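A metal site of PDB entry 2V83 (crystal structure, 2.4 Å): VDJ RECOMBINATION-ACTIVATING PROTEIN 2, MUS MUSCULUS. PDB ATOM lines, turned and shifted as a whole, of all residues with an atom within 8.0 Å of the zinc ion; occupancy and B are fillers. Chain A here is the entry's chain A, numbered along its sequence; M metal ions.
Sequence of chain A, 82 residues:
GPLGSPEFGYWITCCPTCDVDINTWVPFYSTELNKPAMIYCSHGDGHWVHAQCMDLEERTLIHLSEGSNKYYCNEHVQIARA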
ATOM      1  N   CYS A  14      -8.683   3.968  -3.155  1.00  0.00           N
ATOM      2  CA  CYS A  14      -8.020   5.270  -3.086  1.00  0.00           C
ATOM      3  C   CYS A  14      -6.745   5.416  -2.250  1.00  0.00           C
ATOM      4  O   CYS A  14      -6.005   6.386  -2.413  1.00  0.00           O
ATOM      5  CB  CYS A  14      -9.035   6.340  -2.652  1.00  0.00           C
ATOM      6  SG  CYS A  14      -9.443   6.338  -0.896  1.00  0.00           S
ATOM      7  N   CYS A  15      -6.501   4.469  -1.349  1.00  0.00           N
ATOM      8  CA  CYS A  15      -5.308   4.550  -0.515  1.00  0.00           C
ATOM      9  C   CYS A  15      -5.148   3.213   0.203  1.00  0.00           C
ATOM     10  O   CYS A  15      -6.119   2.467   0.366  1.00  0.00           O
ATOM     11  CB  CYS A  15      -5.455   5.695   0.488  1.00  0.00           C
ATOM     12  SG  CYS A  15      -6.740   5.404   1.715  1.00  0.00           S
ATOM     13  N   ILE A  39     -12.792  13.654  -2.904  1.00  0.00           N
ATOM     14  CA  ILE A  39     -12.113  14.925  -2.914  1.00  0.00           C
ATOM     15  C   ILE A  39     -10.818  14.762  -3.700  1.00  0.00           C
ATOM     16  O   ILE A  39     -10.207  13.700  -3.704  1.00  0.00           O
ATOM     17  CB  ILE A  39     -11.818  15.423  -1.498  1.00  0.00           C
ATOM     18  CG1 ILE A  39     -11.292  16.864  -1.557  1.00  0.00           C
ATOM     19  CG2 ILE A  39     -10.854  14.491  -0.801  1.00  0.00           C
ATOM     20  CD1 ILE A  39     -11.287  17.577  -0.235  1.00  0.00           C
ATOM     21  N   TYR A  40     -10.416  15.827  -4.382  1.00  0.00           N
ATOM     22  CA  TYR A  40      -9.226  15.782  -5.203  1.00  0.00           C
ATOM     23  C   TYR A  40      -7.937  16.178  -4.486  1.00  0.00           C
ATOM     24  O   TYR A  40      -7.840  17.270  -3.929  1.00  0.00           O
ATOM     25  CB  TYR A  40      -9.435  16.671  -6.427  1.00  0.00           C
ATOM     26  CG  TYR A  40      -8.354  16.555  -7.461  1.00  0.00           C
ATOM     27  CD1 TYR A  40      -8.296  15.457  -8.310  1.00  0.00           C
ATOM     28  CD2 TYR A  40      -7.375  17.549  -7.601  1.00  0.00           C
ATOM     29  CE1 TYR A  40      -7.291  15.345  -9.269  1.00  0.00           C
ATOM     30  CE2 TYR A  40      -6.371  17.452  -8.550  1.00  0.00           C
ATOM     31  CZ  TYR A  40      -6.337  16.344  -9.387  1.00  0.00           C
ATOM     32  OH  TYR A  40      -5.356  16.236 -10.358  1.00  0.00           O
ATOM     33  N   CYS A  41      -6.956  15.278  -4.491  1.00  0.00           N
ATOM     34  CA  CYS A  41      -5.657  15.546  -3.873  1.00  0.00           C
ATOM     35  C   CYS A  41      -4.783  16.203  -4.940  1.00  0.00           C
ATOM     36  O   CYS A  41      -4.643  15.663  -6.037  1.00  0.00           O
ATOM     37  CB  CYS A  41      -5.014  14.241  -3.405  1.00  0.00           C
ATOM     38  SG  CYS A  41      -3.385  14.459  -2.684  1.00  0.00           S
ATOM     39  N   SER A  42      -4.185  17.353  -4.626  1.00  0.00           N
ATOM     40  CA  SER A  42      -3.354  18.079  -5.595  1.00  0.00           C
ATOM     41  C   SER A  42      -1.910  17.649  -5.698  1.00  0.00           C
ATOM     42  O   SER A  42      -1.115  18.283  -6.379  1.00  0.00           O
ATOM     43  CB  SER A  42      -3.390  19.578  -5.291  1.00  0.00           C
ATOM     44  OG  SER A  42      -4.677  20.118  -5.541  1.00  0.00           O
ATOM     45  N   HIS A  43      -1.560  16.560  -5.004  1.00  0.00           N
ATOM     46  CA  HIS A  43      -0.192  16.069  -5.039  1.00  0.00           C
ATOM     47  C   HIS A  43       0.245  15.571  -6.409  1.00  0.00           C
ATOM     48  O   HIS A  43      -0.470  14.806  -7.066  1.00  0.00           O
ATOM     49  CB  HIS A  43      -0.009  14.952  -4.024  1.00  0.00           C
ATOM     50  CG  HIS A  43       1.406  14.507  -3.874  1.00  0.00           C
ATOM     51  ND1 HIS A  43       1.909  13.396  -4.513  1.00  0.00           N
ATOM     52  CD2 HIS A  43       2.440  15.032  -3.174  1.00  0.00           C
ATOM     53  CE1 HIS A  43       3.185  13.251  -4.213  1.00  0.00           C
ATOM     54  NE2 HIS A  43       3.524  14.241  -3.403  1.00  0.00           N
ATOM     55  N   GLY A  44       1.438  15.991  -6.835  1.00  0.00           N
ATOM     56  CA  GLY A  44       1.958  15.578  -8.116  1.00  0.00           C
ATOM     57  C   GLY A  44       0.952  15.780  -9.221  1.00  0.00           C
ATOM     58  O   GLY A  44       0.396  16.871  -9.370  1.00  0.00           O
ATOM     59  N   GLY A  46      -1.851  14.538  -9.261  1.00  0.00           N
ATOM     60  CA  GLY A  46      -3.147  14.619  -8.636  1.00  0.00           C
ATOM     61  C   GLY A  46      -3.836  13.271  -8.682  1.00  0.00           C
ATOM     62  O   GLY A  46      -3.475  12.402  -9.468  1.00  0.00           O
ATOM     63  N   HIS A  47      -4.831  13.083  -7.822  1.00  0.00           N
ATOM     64  CA  HIS A  47      -5.568  11.842  -7.764  1.00  0.00           C
ATOM     65  C   HIS A  47      -6.762  12.043  -6.844  1.00  0.00           C
ATOM     66  O   HIS A  47      -6.751  12.928  -5.983  1.00  0.00           O
ATOM     67  CB  HIS A  47      -4.677  10.716  -7.234  1.00  0.00           C
ATOM     68  CG  HIS A  47      -4.251  10.906  -5.805  1.00  0.00           C
ATOM     69  ND1 HIS A  47      -4.679  10.083  -4.785  1.00  0.00           N
ATOM     70  CD2 HIS A  47      -3.441  11.836  -5.235  1.00  0.00           C
ATOM     71  CE1 HIS A  47      -4.156  10.490  -3.644  1.00  0.00           C
ATOM     72  NE2 HIS A  47      -3.403  11.553  -3.883  1.00  0.00           N
ATOM     73  N   TRP A  48      -7.792  11.206  -7.036  1.00  0.00           N
ATOM     74  CA  TRP A  48      -9.008  11.263  -6.239  1.00  0.00           C
ATOM     75  C   TRP A  48      -9.031  10.263  -5.084  1.00  0.00           C
ATOM     76  O   TRP A  48      -8.597   9.112  -5.233  1.00  0.00           O
ATOM     77  CB  TRP A  48     -10.239  10.996  -7.113  1.00  0.00           C
ATOM     78  CG  TRP A  48     -10.553  12.049  -8.109  1.00  0.00           C
ATOM     79  CD1 TRP A  48     -10.081  12.139  -9.386  1.00  0.00           C
ATOM     80  CD2 TRP A  48     -11.418  13.185  -7.930  1.00  0.00           C
ATOM     81  NE1 TRP A  48     -10.593  13.260 -10.014  1.00  0.00           N
ATOM     82  CE2 TRP A  48     -11.425  13.912  -9.138  1.00  0.00           C
ATOM     83  CE3 TRP A  48     -12.198  13.645  -6.852  1.00  0.00           C
ATOM     84  CZ2 TRP A  48     -12.167  15.077  -9.302  1.00  0.00           C
ATOM     85  CZ3 TRP A  48     -12.936  14.810  -7.025  1.00  0.00           C
ATOM     86  CH2 TRP A  48     -12.919  15.511  -8.242  1.00  0.00           C
ATOM     87  N   VAL A  49      -9.539  10.684  -3.942  1.00  0.00           N
ATOM     88  CA  VAL A  49      -9.675   9.796  -2.792  1.00  0.00           C
ATOM     89  C   VAL A  49     -11.089   9.904  -2.224  1.00  0.00           C
ATOM     90  O   VAL A  49     -11.791  10.885  -2.458  1.00  0.00           O
ATOM     91  CB  VAL A  49      -8.668  10.153  -1.686  1.00  0.00           C
ATOM     92  CG1 VAL A  49      -7.251   9.856  -2.163  1.00  0.00           C
ATOM     93  CG2 VAL A  49      -8.820  11.626  -1.280  1.00  0.00           C
ATOM     94  N   MET A  54     -10.463   9.454   4.351  1.00  0.00           N
ATOM     95  CA  MET A  54      -9.534  10.451   4.895  1.00  0.00           C
ATOM     96  C   MET A  54      -9.963  10.854   6.297  1.00  0.00           C
ATOM     97  O   MET A  54      -9.284  11.647   6.957  1.00  0.00           O
ATOM     98  CB  MET A  54      -9.498  11.688   3.998  1.00  0.00           C
ATOM     99  CG  MET A  54      -9.089  11.411   2.569  1.00  0.00           C
ATOM    100  SD  MET A  54      -7.384  10.845   2.420  1.00  0.00           S
ATOM    101  CE  MET A  54      -7.584   9.100   2.052  1.00  0.00           C
ATOM    102  N   TYR A  71      -6.359  20.579  -1.579  1.00  0.00           N
ATOM    103  CA  TYR A  71      -6.426  19.511  -0.606  1.00  0.00           C
ATOM    104  C   TYR A  71      -5.339  18.476  -0.863  1.00  0.00           C
ATOM    105  O   TYR A  71      -5.025  18.152  -2.014  1.00  0.00           O
ATOM    106  CB  TYR A  71      -7.795  18.827  -0.635  1.00  0.00           C
ATOM    107  CG  TYR A  71      -7.893  17.657   0.318  1.00  0.00           C
ATOM    108  CD1 TYR A  71      -7.867  16.343  -0.146  1.00  0.00           C
ATOM    109  CD2 TYR A  71      -7.942  17.861   1.699  1.00  0.00           C
ATOM    110  CE1 TYR A  71      -7.883  15.267   0.751  1.00  0.00           C
ATOM    111  CE2 TYR A  71      -7.951  16.799   2.588  1.00  0.00           C
ATOM    112  CZ  TYR A  71      -7.924  15.506   2.112  1.00  0.00           C
ATOM    113  OH  TYR A  71      -7.894  14.459   3.007  1.00  0.00           O
ATOM    114  N   TYR A  72      -4.762  17.966   0.213  1.00  0.00           N
ATOM    115  CA  TYR A  72      -3.750  16.926   0.109  1.00  0.00           C
ATOM    116  C   TYR A  72      -4.189  15.812   1.030  1.00  0.00           C
ATOM    117  O   TYR A  72      -4.519  16.067   2.188  1.00  0.00           O
ATOM    118  CB  TYR A  72      -2.374  17.464   0.515  1.00  0.00           C
ATOM    119  CG  TYR A  72      -1.867  18.531  -0.416  1.00  0.00           C
ATOM    120  CD1 TYR A  72      -2.177  19.869  -0.210  1.00  0.00           C
ATOM    121  CD2 TYR A  72      -1.139  18.188  -1.559  1.00  0.00           C
ATOM    122  CE1 TYR A  72      -1.789  20.832  -1.113  1.00  0.00           C
ATOM    123  CE2 TYR A  72      -0.751  19.160  -2.474  1.00  0.00           C
ATOM    124  CZ  TYR A  72      -1.077  20.485  -2.241  1.00  0.00           C
ATOM    125  OH  TYR A  72      -0.709  21.480  -3.122  1.00  0.00           O
ATOM    126  N   CYS A  73      -4.232  14.590   0.495  1.00  0.00           N
ATOM    127  CA  CYS A  73      -4.661  13.434   1.280  1.00  0.00           C
ATOM    128  C   CYS A  73      -3.686  13.122   2.411  1.00  0.00           C
ATOM    129  O   CYS A  73      -2.532  13.555   2.397  1.00  0.00           O
ATOM    130  CB  CYS A  73      -4.824  12.202   0.380  1.00  0.00           C
ATOM    131  SG  CYS A  73      -3.274  11.528  -0.246  1.00  0.00           S
ATOM    132  N   ASN A  74      -4.161  12.380   3.393  1.00  0.00           N
ATOM    133  CA  ASN A  74      -3.362  12.017   4.555  1.00  0.00           C
ATOM    134  C   ASN A  74      -2.002  11.427   4.189  1.00  0.00           C
ATOM    135  O   ASN A  74      -1.061  11.485   4.994  1.00  0.00           O
ATOM    136  CB  ASN A  74      -4.155  11.064   5.444  1.00  0.00           C
ATOM    137  CG  ASN A  74      -5.499  11.629   5.851  1.00  0.00           C
ATOM    138  OD1 ASN A  74      -5.596  12.800   6.213  1.00  0.00           O
ATOM    139  ND2 ASN A  74      -6.542  10.821   5.795  1.00  0.00           N
ATOM    140  N   GLU A  75      -1.883  10.863   2.994  1.00  0.00           N
ATOM    141  CA  GLU A  75      -0.626  10.277   2.547  1.00  0.00           C
ATOM    142  C   GLU A  75       0.358  11.321   2.019  1.00  0.00           C
ATOM    143  O   GLU A  75       1.562  11.170   2.152  1.00  0.00           O
ATOM    144  CB  GLU A  75      -0.859   9.247   1.435  1.00  0.00           C
ATOM    145  CG  GLU A  75      -1.336   7.883   1.900  1.00  0.00           C
ATOM    146  CD  GLU A  75      -1.512   6.923   0.745  1.00  0.00           C
ATOM    147  OE1 GLU A  75      -0.511   6.409   0.228  1.00  0.00           O
ATOM    148  OE2 GLU A  75      -2.674   6.700   0.355  1.00  0.00           O
ATOM    149  N   HIS A  76      -0.177  12.374   1.417  1.00  0.00           N
ATOM    150  CA  HIS A  76       0.661  13.409   0.810  1.00  0.00           C
ATOM    151  C   HIS A  76       0.770  14.746   1.513  1.00  0.00           C
ATOM    152  O   HIS A  76       1.544  15.602   1.074  1.00  0.00           O
ATOM    153  CB  HIS A  76       0.170  13.660  -0.621  1.00  0.00           C
ATOM    154  CG  HIS A  76       0.245  12.460  -1.510  1.00  0.00           C
ATOM    155  ND1 HIS A  76      -0.603  12.270  -2.574  1.00  0.00           N
ATOM    156  CD2 HIS A  76       1.090  11.403  -1.504  1.00  0.00           C
ATOM    157  CE1 HIS A  76      -0.281  11.153  -3.186  1.00  0.00           C
ATOM    158  NE2 HIS A  76       0.745  10.606  -2.561  1.00  0.00           N
ATOM    159  N   VAL A  77       0.027  14.956   2.590  1.00  0.00           N
ATOM    160  CA  VAL A  77       0.063  16.264   3.238  1.00  0.00           C
ATOM    161  C   VAL A  77       1.444  16.833   3.545  1.00  0.00           C
ATOM    162  O   VAL A  77       1.629  18.044   3.483  1.00  0.00           O
ATOM    163  CB  VAL A  77      -0.734  16.300   4.543  1.00  0.00           C
ATOM    164  CG1 VAL A  77      -1.470  17.624   4.639  1.00  0.00           C
ATOM    165  CG2 VAL A  77      -1.696  15.139   4.602  1.00  0.00           C
HETATM  166 ZN    ZN M   1      -2.691  12.387  -2.269  1.00  0.00          ZN
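The side-chain sulfur (SG) of Cys 73 lies close to the backbone NH (N) of Glu 75, 3.6 Å away.
A ring nitrogen (ND1) of His 76 sits close to a ring nitrogen (ND1) of His 43, 3.4 Å away.
The backbone NH (N) of His 43 sits close to the side-chain sulfur (SG) of Cys 41.
Within 4 Å of the zinc ion: Cys 41, His 47, Cys 73 and His 76.
Along chain A the residues within 4 Å of the zinc ion span positions 41 to 76.
The nearest printed residue that does not touch the zinc ion is His 43 (4.1 Å).
NE2 of His 47 binds the zinc ion.
ND1 of His 76 binds the zinc ion (2.1 Å).
SG of Cys 41 binds the zinc ion (2.2 Å).
The zinc ion is bound by SG of Cys 73.
The zinc ion has four donor atoms within binding distance.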
